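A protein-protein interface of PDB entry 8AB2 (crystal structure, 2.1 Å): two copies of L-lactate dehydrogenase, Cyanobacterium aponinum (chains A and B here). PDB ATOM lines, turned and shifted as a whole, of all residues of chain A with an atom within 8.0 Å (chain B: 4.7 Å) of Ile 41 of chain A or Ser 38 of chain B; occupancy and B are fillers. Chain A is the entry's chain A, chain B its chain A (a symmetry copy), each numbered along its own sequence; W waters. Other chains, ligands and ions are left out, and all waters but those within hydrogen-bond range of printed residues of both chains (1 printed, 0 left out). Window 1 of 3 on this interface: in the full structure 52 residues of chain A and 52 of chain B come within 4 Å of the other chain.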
ATOM      1  N   ALA A  34     -36.565  16.981 -20.786  1.00  0.00           N
ATOM      2  CA  ALA A  34     -36.631  16.131 -21.970  1.00  0.00           C
ATOM      3  C   ALA A  34     -36.637  16.968 -23.242  1.00  0.00           C
ATOM      4  O   ALA A  34     -35.956  16.633 -24.219  1.00  0.00           O
ATOM      5  CB  ALA A  34     -37.866  15.233 -21.909  1.00  0.00           C
ATOM      6  N   CYS A  35     -37.402  18.064 -23.248  1.00  0.00           N
ATOM      7  CA  CYS A  35     -37.370  18.982 -24.383  1.00  0.00           C
ATOM      8  C   CYS A  35     -35.966  19.524 -24.613  1.00  0.00           C
ATOM      9  O   CYS A  35     -35.484  19.558 -25.750  1.00  0.00           O
ATOM     10  CB  CYS A  35     -38.349  20.135 -24.158  1.00  0.00           C
ATOM     11  SG  CYS A  35     -40.095  19.677 -24.166  1.00  0.00           S
ATOM     12  N   ALA A  36     -35.293  19.946 -23.540  1.00  0.00           N
ATOM     13  CA  ALA A  36     -33.969  20.543 -23.676  1.00  0.00           C
ATOM     14  C   ALA A  36     -32.967  19.539 -24.232  1.00  0.00           C
ATOM     15  O   ALA A  36     -32.217  19.848 -25.165  1.00  0.00           O
ATOM     16  CB  ALA A  36     -33.498  21.085 -22.325  1.00  0.00           C
ATOM     17  N   TYR A  37     -32.948  18.325 -23.675  1.00  0.00           N
ATOM     18  CA  TYR A  37     -32.014  17.305 -24.143  1.00  0.00           C
ATOM     19  C   TYR A  37     -32.226  17.001 -25.621  1.00  0.00           C
ATOM     20  O   TYR A  37     -31.261  16.882 -26.385  1.00  0.00           O
ATOM     21  CB  TYR A  37     -32.170  16.034 -23.307  1.00  0.00           C
ATOM     22  CG  TYR A  37     -30.970  15.112 -23.328  1.00  0.00           C
ATOM     23  CD1 TYR A  37     -29.691  15.604 -23.558  1.00  0.00           C
ATOM     24  CD2 TYR A  37     -31.117  13.746 -23.118  1.00  0.00           C
ATOM     25  CE1 TYR A  37     -28.592  14.761 -23.573  1.00  0.00           C
ATOM     26  CE2 TYR A  37     -30.029  12.898 -23.132  1.00  0.00           C
ATOM     27  CZ  TYR A  37     -28.769  13.408 -23.360  1.00  0.00           C
ATOM     28  OH  TYR A  37     -27.683  12.564 -23.374  1.00  0.00           O
ATOM     29  N   SER A  38     -33.486  16.884 -26.044  1.00  0.00           N
ATOM     30  CA  SER A  38     -33.778  16.607 -27.446  1.00  0.00           C
ATOM     31  C   SER A  38     -33.369  17.773 -28.338  1.00  0.00           C
ATOM     32  O   SER A  38     -32.719  17.581 -29.372  1.00  0.00           O
ATOM     33  CB  SER A  38     -35.265  16.295 -27.617  1.00  0.00           C
ATOM     34  OG  SER A  38     -35.619  16.250 -28.988  1.00  0.00           O
ATOM     35  N   MET A  39     -33.741  18.996 -27.951  1.00  0.00           N
ATOM     36  CA  MET A  39     -33.454  20.154 -28.791  1.00  0.00           C
ATOM     37  C   MET A  39     -31.960  20.447 -28.864  1.00  0.00           C
ATOM     38  O   MET A  39     -31.497  21.047 -29.841  1.00  0.00           O
ATOM     39  CB  MET A  39     -34.219  21.373 -28.276  1.00  0.00           C
ATOM     40  CG  MET A  39     -35.732  21.235 -28.404  1.00  0.00           C
ATOM     41  SD  MET A  39     -36.634  22.492 -27.485  1.00  0.00           S
ATOM     42  CE  MET A  39     -38.317  21.913 -27.683  1.00  0.00           C
ATOM     43  N   LEU A  40     -31.194  20.034 -27.851  1.00  0.00           N
ATOM     44  CA  LEU A  40     -29.743  20.176 -27.919  1.00  0.00           C
ATOM     45  C   LEU A  40     -29.139  19.149 -28.867  1.00  0.00           C
ATOM     46  O   LEU A  40     -28.306  19.486 -29.718  1.00  0.00           O
ATOM     47  CB  LEU A  40     -29.136  20.040 -26.521  1.00  0.00           C
ATOM     48  CG  LEU A  40     -29.376  21.197 -25.550  1.00  0.00           C
ATOM     49  CD1 LEU A  40     -28.953  20.809 -24.142  1.00  0.00           C
ATOM     50  CD2 LEU A  40     -28.633  22.439 -26.008  1.00  0.00           C
ATOM     51  N   ILE A  41     -29.550  17.884 -28.736  1.00  0.00           N
ATOM     52  CA  ILE A  41     -29.014  16.832 -29.594  1.00  0.00           C
ATOM     53  C   ILE A  41     -29.372  17.095 -31.051  1.00  0.00           C
ATOM     54  O   ILE A  41     -28.547  16.903 -31.954  1.00  0.00           O
ATOM     55  CB  ILE A  41     -29.518  15.454 -29.123  1.00  0.00           C
ATOM     56  CG1 ILE A  41     -28.976  15.134 -27.729  1.00  0.00           C
ATOM     57  CG2 ILE A  41     -29.119  14.368 -30.111  1.00  0.00           C
ATOM     58  CD1 ILE A  41     -29.505  13.839 -27.150  1.00  0.00           C
ATOM     59  N   GLN A  42     -30.595  17.553 -31.307  1.00  0.00           N
ATOM     60  CA  GLN A  42     -31.052  17.805 -32.667  1.00  0.00           C
ATOM     61  C   GLN A  42     -30.691  19.199 -33.169  1.00  0.00           C
ATOM     62  O   GLN A  42     -31.082  19.558 -34.285  1.00  0.00           O
ATOM     63  CB  GLN A  42     -32.567  17.583 -32.760  1.00  0.00           C
ATOM     64  CG  GLN A  42     -33.003  16.211 -32.251  1.00  0.00           C
ATOM     65  CD  GLN A  42     -34.364  15.788 -32.765  1.00  0.00           C
ATOM     66  OE1 GLN A  42     -34.559  15.620 -33.968  1.00  0.00           O
ATOM     67  NE2 GLN A  42     -35.312  15.605 -31.854  1.00  0.00           N
ATOM     68  N   ASP A  43     -29.961  19.986 -32.373  1.00  0.00           N
ATOM     69  CA  ASP A  43     -29.376  21.257 -32.813  1.00  0.00           C
ATOM     70  C   ASP A  43     -30.443  22.228 -33.320  1.00  0.00           C
ATOM     71  O   ASP A  43     -30.352  22.768 -34.425  1.00  0.00           O
ATOM     72  CB  ASP A  43     -28.301  21.018 -33.879  1.00  0.00           C
ATOM     73  CG  ASP A  43     -27.477  22.261 -34.168  1.00  0.00           C
ATOM     74  OD1 ASP A  43     -27.491  23.192 -33.336  1.00  0.00           O
ATOM     75  OD2 ASP A  43     -26.822  22.308 -35.229  1.00  0.00           O
ATOM     76  N   CYS A  44     -31.461  22.465 -32.491  1.00  0.00           N
ATOM     77  CA  CYS A  44     -32.545  23.354 -32.894  1.00  0.00           C
ATOM     78  C   CYS A  44     -32.139  24.821 -32.815  1.00  0.00           C
ATOM     79  O   CYS A  44     -32.465  25.605 -33.714  1.00  0.00           O
ATOM     80  CB  CYS A  44     -33.782  23.107 -32.031  1.00  0.00           C
ATOM     81  SG  CYS A  44     -34.522  21.478 -32.240  1.00  0.00           S
ATOM     82  N   LEU A  48     -29.942  28.616 -26.190  1.00  0.00           N
ATOM     83  CA  LEU A  48     -31.089  28.050 -25.487  1.00  0.00           C
ATOM     84  C   LEU A  48     -31.019  28.452 -24.023  1.00  0.00           C
ATOM     85  O   LEU A  48     -30.039  28.141 -23.337  1.00  0.00           O
ATOM     86  CB  LEU A  48     -31.123  26.524 -25.628  1.00  0.00           C
ATOM     87  CG  LEU A  48     -32.284  25.795 -24.950  1.00  0.00           C
ATOM     88  CD1 LEU A  48     -33.618  26.313 -25.467  1.00  0.00           C
ATOM     89  CD2 LEU A  48     -32.168  24.296 -25.170  1.00  0.00           C
ATOM     90  N   PHE A  65     -25.663  19.637 -19.132  1.00  0.00           N
ATOM     91  CA  PHE A  65     -25.817  19.858 -20.566  1.00  0.00           C
ATOM     92  C   PHE A  65     -24.547  20.448 -21.169  1.00  0.00           C
ATOM     93  O   PHE A  65     -24.061  19.979 -22.206  1.00  0.00           O
ATOM     94  CB  PHE A  65     -27.007  20.782 -20.831  1.00  0.00           C
ATOM     95  CG  PHE A  65     -28.351  20.127 -20.649  1.00  0.00           C
ATOM     96  CD1 PHE A  65     -28.596  18.859 -21.150  1.00  0.00           C
ATOM     97  CD2 PHE A  65     -29.372  20.788 -19.985  1.00  0.00           C
ATOM     98  CE1 PHE A  65     -29.835  18.262 -20.989  1.00  0.00           C
ATOM     99  CE2 PHE A  65     -30.612  20.196 -19.818  1.00  0.00           C
ATOM    100  CZ  PHE A  65     -30.842  18.932 -20.320  1.00  0.00           C
ATOM    101  N   GLY A  68     -21.568  18.033 -21.741  1.00  0.00           N
ATOM    102  CA  GLY A  68     -21.714  17.065 -22.811  1.00  0.00           C
ATOM    103  C   GLY A  68     -21.808  17.644 -24.204  1.00  0.00           C
ATOM    104  O   GLY A  68     -21.812  16.885 -25.177  1.00  0.00           O
ATOM    105  N   MET A  69     -21.871  18.971 -24.316  1.00  0.00           N
ATOM    106  CA  MET A  69     -22.008  19.615 -25.620  1.00  0.00           C
ATOM    107  C   MET A  69     -20.946  19.223 -26.647  1.00  0.00           C
ATOM    108  O   MET A  69     -21.295  19.139 -27.838  1.00  0.00           O
ATOM    109  CB  MET A  69     -22.024  21.140 -25.444  1.00  0.00           C
ATOM    110  CG  MET A  69     -23.262  21.689 -24.753  1.00  0.00           C
ATOM    111  SD  MET A  69     -24.802  21.227 -25.572  1.00  0.00           S
ATOM    112  CE  MET A  69     -24.487  21.788 -27.241  1.00  0.00           C
ATOM    113  N   PHE A  71     -19.952  16.616 -27.787  1.00  0.00           N
ATOM    114  CA  PHE A  71     -20.332  15.451 -28.575  1.00  0.00           C
ATOM    115  C   PHE A  71     -21.449  15.729 -29.575  1.00  0.00           C
ATOM    116  O   PHE A  71     -21.748  14.858 -30.398  1.00  0.00           O
ATOM    117  CB  PHE A  71     -20.752  14.306 -27.650  1.00  0.00           C
ATOM    118  CG  PHE A  71     -19.656  13.835 -26.739  1.00  0.00           C
ATOM    119  CD1 PHE A  71     -18.635  13.035 -27.221  1.00  0.00           C
ATOM    120  CD2 PHE A  71     -19.644  14.199 -25.404  1.00  0.00           C
ATOM    121  CE1 PHE A  71     -17.622  12.600 -26.388  1.00  0.00           C
ATOM    122  CE2 PHE A  71     -18.634  13.769 -24.566  1.00  0.00           C
ATOM    123  CZ  PHE A  71     -17.622  12.967 -25.059  1.00  0.00           C
ATOM    124  N   ILE A  72     -22.060  16.909 -29.531  1.00  0.00           N
ATOM    125  CA  ILE A  72     -23.161  17.259 -30.428  1.00  0.00           C
ATOM    126  C   ILE A  72     -22.859  18.626 -31.037  1.00  0.00           C
ATOM    127  O   ILE A  72     -21.869  19.259 -30.641  1.00  0.00           O
ATOM    128  CB  ILE A  72     -24.506  17.243 -29.681  1.00  0.00           C
ATOM    129  CG1 ILE A  72     -24.440  18.113 -28.426  1.00  0.00           C
ATOM    130  CG2 ILE A  72     -24.909  15.814 -29.336  1.00  0.00           C
ATOM    131  CD1 ILE A  72     -25.754  18.188 -27.672  1.00  0.00           C
ATOM    132  N   PRO A  73     -23.636  19.109 -32.007  1.00  0.00           N
ATOM    133  CA  PRO A  73     -23.392  20.450 -32.527  1.00  0.00           C
ATOM    134  C   PRO A  73     -23.494  21.483 -31.425  1.00  0.00           C
ATOM    135  O   PRO A  73     -24.240  21.301 -30.445  1.00  0.00           O
ATOM    136  CB  PRO A  73     -24.501  20.629 -33.575  1.00  0.00           C
ATOM    137  CG  PRO A  73     -24.779  19.257 -34.043  1.00  0.00           C
ATOM    138  CD  PRO A  73     -24.617  18.377 -32.835  1.00  0.00           C
ATOM    139  N   THR A  75     -24.358  24.564 -28.993  1.00  0.00           N
ATOM    140  CA  THR A  75     -25.490  25.400 -28.620  1.00  0.00           C
ATOM    141  C   THR A  75     -25.121  26.135 -27.340  1.00  0.00           C
ATOM    142  O   THR A  75     -24.645  25.514 -26.384  1.00  0.00           O
ATOM    143  CB  THR A  75     -26.769  24.580 -28.409  1.00  0.00           C
ATOM    144  OG1 THR A  75     -27.155  23.956 -29.641  1.00  0.00           O
ATOM    145  CG2 THR A  75     -27.900  25.475 -27.924  1.00  0.00           C
ATOM    146  N   TYR A 250     -40.480  11.937 -22.544  1.00  0.00           N
ATOM    147  CA  TYR A 250     -39.701  11.708 -23.756  1.00  0.00           C
ATOM    148  C   TYR A 250     -40.559  11.848 -25.009  1.00  0.00           C
ATOM    149  O   TYR A 250     -40.117  12.433 -26.004  1.00  0.00           O
ATOM    150  CB  TYR A 250     -39.042  10.332 -23.698  1.00  0.00           C
ATOM    151  CG  TYR A 250     -38.101  10.169 -22.523  1.00  0.00           C
ATOM    152  CD1 TYR A 250     -36.947  10.933 -22.425  1.00  0.00           C
ATOM    153  CD2 TYR A 250     -38.367   9.253 -21.514  1.00  0.00           C
ATOM    154  CE1 TYR A 250     -36.080  10.791 -21.355  1.00  0.00           C
ATOM    155  CE2 TYR A 250     -37.507   9.102 -20.441  1.00  0.00           C
ATOM    156  CZ  TYR A 250     -36.365   9.874 -20.367  1.00  0.00           C
ATOM    157  OH  TYR A 250     -35.506   9.730 -19.302  1.00  0.00           O
ATOM    158  N   THR A 257     -40.157  19.147 -29.914  1.00  0.00           N
ATOM    159  CA  THR A 257     -39.017  19.446 -30.775  1.00  0.00           C
ATOM    160  C   THR A 257     -39.429  19.473 -32.242  1.00  0.00           C
ATOM    161  O   THR A 257     -38.969  20.326 -33.010  1.00  0.00           O
ATOM    162  CB  THR A 257     -37.908  18.417 -30.548  1.00  0.00           C
ATOM    163  OG1 THR A 257     -37.502  18.440 -29.174  1.00  0.00           O
ATOM    164  CG2 THR A 257     -36.706  18.716 -31.431  1.00  0.00           C
ATOM    165  N   ALA B  34     -30.785   8.474 -19.774  1.00  0.00           N
ATOM    166  CA  ALA B  34     -30.138   9.478 -20.612  1.00  0.00           C
ATOM    167  C   ALA B  34     -29.428   8.827 -21.792  1.00  0.00           C
ATOM    168  O   ALA B  34     -29.503   9.324 -22.922  1.00  0.00           O
ATOM    169  CB  ALA B  34     -29.159  10.307 -19.783  1.00  0.00           C
ATOM    170  N   CYS B  35     -28.731   7.713 -21.546  1.00  0.00           N
ATOM    171  CA  CYS B  35     -28.122   6.965 -22.641  1.00  0.00           C
ATOM    172  C   CYS B  35     -29.170   6.517 -23.651  1.00  0.00           C
ATOM    173  O   CYS B  35     -28.977   6.662 -24.864  1.00  0.00           O
ATOM    174  CB  CYS B  35     -27.365   5.752 -22.098  1.00  0.00           C
ATOM    175  SG  CYS B  35     -25.898   6.138 -21.118  1.00  0.00           S
ATOM    176  N   ALA B  36     -30.291   5.976 -23.167  1.00  0.00           N
ATOM    177  CA  ALA B  36     -31.318   5.458 -24.063  1.00  0.00           C
ATOM    178  C   ALA B  36     -31.914   6.570 -24.919  1.00  0.00           C
ATOM    179  O   ALA B  36     -32.046   6.425 -26.139  1.00  0.00           O
ATOM    180  CB  ALA B  36     -32.409   4.752 -23.258  1.00  0.00           C
ATOM    181  N   TYR B  37     -32.274   7.694 -24.292  1.00  0.00           N
ATOM    182  CA  TYR B  37     -32.860   8.806 -25.035  1.00  0.00           C
ATOM    183  C   TYR B  37     -31.912   9.305 -26.117  1.00  0.00           C
ATOM    184  O   TYR B  37     -32.332   9.569 -27.250  1.00  0.00           O
ATOM    185  CB  TYR B  37     -33.219   9.940 -24.074  1.00  0.00           C
ATOM    186  CG  TYR B  37     -34.264  10.904 -24.596  1.00  0.00           C
ATOM    187  CD1 TYR B  37     -35.207  10.500 -25.533  1.00  0.00           C
ATOM    188  CD2 TYR B  37     -34.305  12.218 -24.150  1.00  0.00           C
ATOM    189  CE1 TYR B  37     -36.166  11.381 -26.007  1.00  0.00           C
ATOM    190  CE2 TYR B  37     -35.255  13.105 -24.618  1.00  0.00           C
ATOM    191  CZ  TYR B  37     -36.183  12.681 -25.546  1.00  0.00           C
ATOM    192  OH  TYR B  37     -37.131  13.563 -26.014  1.00  0.00           O
ATOM    193  N   SER B  38     -30.624   9.430 -25.790  1.00  0.00           N
ATOM    194  CA  SER B  38     -29.647   9.889 -26.772  1.00  0.00           C
ATOM    195  C   SER B  38     -29.476   8.875 -27.897  1.00  0.00           C
ATOM    196  O   SER B  38     -29.489   9.237 -29.080  1.00  0.00           O
ATOM    197  CB  SER B  38     -28.308  10.162 -26.086  1.00  0.00           C
ATOM    198  OG  SER B  38     -27.286  10.384 -27.040  1.00  0.00           O
ATOM    199  N   MET B  39     -29.316   7.597 -27.548  1.00  0.00           N
ATOM    200  CA  MET B  39     -29.069   6.580 -28.566  1.00  0.00           C
ATOM    201  C   MET B  39     -30.286   6.361 -29.456  1.00  0.00           C
ATOM    202  O   MET B  39     -30.139   5.923 -30.603  1.00  0.00           O
ATOM    203  CB  MET B  39     -28.643   5.272 -27.902  1.00  0.00           C
ATOM    204  CG  MET B  39     -27.297   5.365 -27.191  1.00  0.00           C
ATOM    205  SD  MET B  39     -26.968   3.955 -26.121  1.00  0.00           S
ATOM    206  CE  MET B  39     -25.458   4.490 -25.316  1.00  0.00           C
ATOM    207  N   LEU B  40     -31.487   6.659 -28.956  1.00  0.00           N
ATOM    208  CA  LEU B  40     -32.677   6.586 -29.797  1.00  0.00           C
ATOM    209  C   LEU B  40     -32.730   7.760 -30.768  1.00  0.00           C
ATOM    210  O   LEU B  40     -32.973   7.579 -31.968  1.00  0.00           O
ATOM    211  CB  LEU B  40     -33.935   6.548 -28.929  1.00  0.00           C
ATOM    212  CG  LEU B  40     -34.198   5.259 -28.151  1.00  0.00           C
ATOM    213  CD1 LEU B  40     -35.316   5.463 -27.141  1.00  0.00           C
ATOM    214  CD2 LEU B  40     -34.536   4.124 -29.101  1.00  0.00           C
ATOM    215  N   ILE B  41     -32.501   8.975 -30.263  1.00  0.00           N
ATOM    216  CA  ILE B  41     -32.545  10.159 -31.117  1.00  0.00           C
ATOM    217  C   ILE B  41     -31.461  10.088 -32.186  1.00  0.00           C
ATOM    218  O   ILE B  41     -31.692  10.437 -33.350  1.00  0.00           O
ATOM    219  CB  ILE B  41     -32.421  11.436 -30.264  1.00  0.00           C
ATOM    220  CG1 ILE B  41     -33.631  11.579 -29.338  1.00  0.00           C
ATOM    221  CG2 ILE B  41     -32.283  12.664 -31.149  1.00  0.00           C
ATOM    222  CD1 ILE B  41     -33.539  12.757 -28.391  1.00  0.00           C
ATOM    223  N   GLN B  42     -30.271   9.622 -31.818  1.00  0.00           N
ATOM    224  CA  GLN B  42     -29.154   9.544 -32.751  1.00  0.00           C
ATOM    225  C   GLN B  42     -29.139   8.250 -33.559  1.00  0.00           C
ATOM    226  O   GLN B  42     -28.204   8.037 -34.337  1.00  0.00           O
ATOM    227  CB  GLN B  42     -27.829   9.717 -31.999  1.00  0.00           C
ATOM    228  CG  GLN B  42     -27.784  10.984 -31.150  1.00  0.00           C
ATOM    229  CD  GLN B  42     -26.374  11.420 -30.803  1.00  0.00           C
ATOM    230  OE1 GLN B  42     -25.581  11.748 -31.683  1.00  0.00           O
ATOM    231  NE2 GLN B  42     -26.059  11.436 -29.514  1.00  0.00           N
ATOM    232  N   GLY B 253     -24.215  10.437 -20.805  1.00  0.00           N
ATOM    233  CA  GLY B 253     -25.036   9.795 -21.820  1.00  0.00           C
ATOM    234  C   GLY B 253     -24.569  10.108 -23.228  1.00  0.00           C
ATOM    235  O   GLY B 253     -24.552   9.230 -24.095  1.00  0.00           O
ATOM    236  N   LEU B 254     -24.174  11.359 -23.473  1.00  0.00           N
ATOM    237  CA  LEU B 254     -23.666  11.729 -24.791  1.00  0.00           C
ATOM    238  C   LEU B 254     -22.292  11.120 -25.043  1.00  0.00           C
ATOM    239  O   LEU B 254     -21.997  10.686 -26.163  1.00  0.00           O
ATOM    240  CB  LEU B 254     -23.615  13.250 -24.923  1.00  0.00           C
ATOM    241  CG  LEU B 254     -24.982  13.937 -24.990  1.00  0.00           C
ATOM    242  CD1 LEU B 254     -24.836  15.450 -24.983  1.00  0.00           C
ATOM    243  CD2 LEU B 254     -25.741  13.475 -26.224  1.00  0.00           C
ATOM    244  N   THR B 257     -22.831   7.464 -25.825  1.00  0.00           N
ATOM    245  CA  THR B 257     -23.331   7.336 -27.190  1.00  0.00           C
ATOM    246  C   THR B 257     -22.206   7.498 -28.205  1.00  0.00           C
ATOM    247  O   THR B 257     -22.156   6.780 -29.211  1.00  0.00           O
ATOM    248  CB  THR B 257     -24.433   8.366 -27.442  1.00  0.00           C
ATOM    249  OG1 THR B 257     -25.502   8.167 -26.508  1.00  0.00           O
ATOM    250  CG2 THR B 257     -24.975   8.242 -28.859  1.00  0.00           C
HETATM  251  O   HOH W   1     -23.193  13.988 -32.624  1.00  0.00           O
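The backbone carbonyl oxygen (O) of Tyr 250 of chain A lies within hydrogen-bond range of the side-chain hydroxyl (OH) of Tyr 37 of chain B, at 3.2 Å.
Among the printed residues, pairs that only touch across the chains: Ala 34 of chain A with Tyr 37 of chain B, Tyr 37 of chain A with Ala 34 of chain B, Tyr 37 of chain A with Tyr 37 of chain B, Tyr 37 of chain A with Ser 38 of chain B, Tyr 37 of chain A with Gly 253 of chain B, Tyr 37 of chain A with Leu 254 of chain B, Ser 38 of chain A with Tyr 37 of chain B, Ser 38 of chain A with Ile 41 of chain B, Ile 41 of chain A with Ser 38 of chain B, Ile 41 of chain A with Ile 41 of chain B, Ile 41 of chain A with Gln 42 of chain B, Ile 41 of chain A with Leu 254 of chain B, Gln 42 of chain A with Ile 41 of chain B, Gly 68 of chain A with Leu 254 of chain B, Phe 71 of chain A with Leu 254 of chain B and Ile 72 of chain A with Leu 254 of chain B.
Water W1 lies within hydrogen-bond range of O of Phe 71 of chain A (2.8 Å) and OE1 of Gln 42 of chain B (3.4 Å).
Of the 21 printed residues of chain A, 9 touch a printed residue of chain B.
Printed residues of chain A that touch a printed residue of chain B: Ala 34, Tyr 37, Ser 38, Ile 41, Gln 42, Gly 68, Phe 71, Ile 72 and Tyr 250.
Printed residues of chain B that touch a printed residue of chain A: Ala 34, Tyr 37, Ser 38, Ile 41, Gln 42, Gly 253 and Leu 254.
Among the printed residues, 17 pairs touch across the chains.
Tyr 37 of chain B touches its own counterpart, Tyr 37 of chain A.
Tyr 37 of chain A touches Ser 38 of chain B, and with the chains exchanged Ser 38 of chain A touches Tyr 37 of chain B.
Ser 38 of chain A touches Ile 41 of chain B, and with the chains exchanged Ile 41 of chain A touches Ser 38 of chain B.
Ile 41 of chain A touches its own counterpart, Ile 41 of chain B.
Of chain B, only Ser 38 (3.97 Å), Ile 41 (3.7 Å), Gln 42 (3.8 Å) and Leu 254 (3.9 Å) come within 4 Å of Ile 41 of chain A.
Of the printed residues of chain B, Gln 42 of chain A touches Ile 41.
Of the printed residues of chain B, Gly 68 of chain A touches Leu 254.
Printed residues of chain B within 4 Å of Tyr 250 of chain A: Tyr 37 (3.2 Å).
Printed residues of chain A within 4 Å of Tyr 37 of chain B: Ala 34 (3.6 Å), Tyr 37 (3.7 Å), Ser 38 (3.7 Å) and Tyr 250 (3.2 Å).
Ser 38 of chain B touches two residues of chain A.
Of the printed residues of chain A, Ile 41 of chain B touches Ser 38, Ile 41 and Gln 42.
The nearest residue of chain A that does not touch Ser 38 of chain B is Ile 72 of chain A (6.4 Å).
The nearest printed residue of chain B that does not touch Tyr 250 of chain A is Ala 34 of chain B (4.9 Å).
The side-chain hydroxyl of Ser 38 of chain A sits at hydrogen-bond distance from the side-chain amide nitrogen of Gln 42 of chain A (3.0 Å).
The side-chain hydroxyl (OG) of Ser 38 of chain A lies within hydrogen-bond range of the side-chain hydroxyl (OG1) of Thr 257 of chain A (2.9 Å).
NE2 of Gln 42 of chain B sits at hydrogen-bond distance from OG of Ser 38 of chain B, 3.0 Å away.
The side-chain hydroxyl (OG) of Ser 38 of chain B lies within hydrogen-bond range of the side-chain hydroxyl (OG1) of Thr 257 of chain B, at 2.9 Å.
The side-chain hydroxyl of Thr 257 of chain B sits at hydrogen-bond distance from the backbone carbonyl oxygen of Gly 253 of chain B (2.8 Å).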
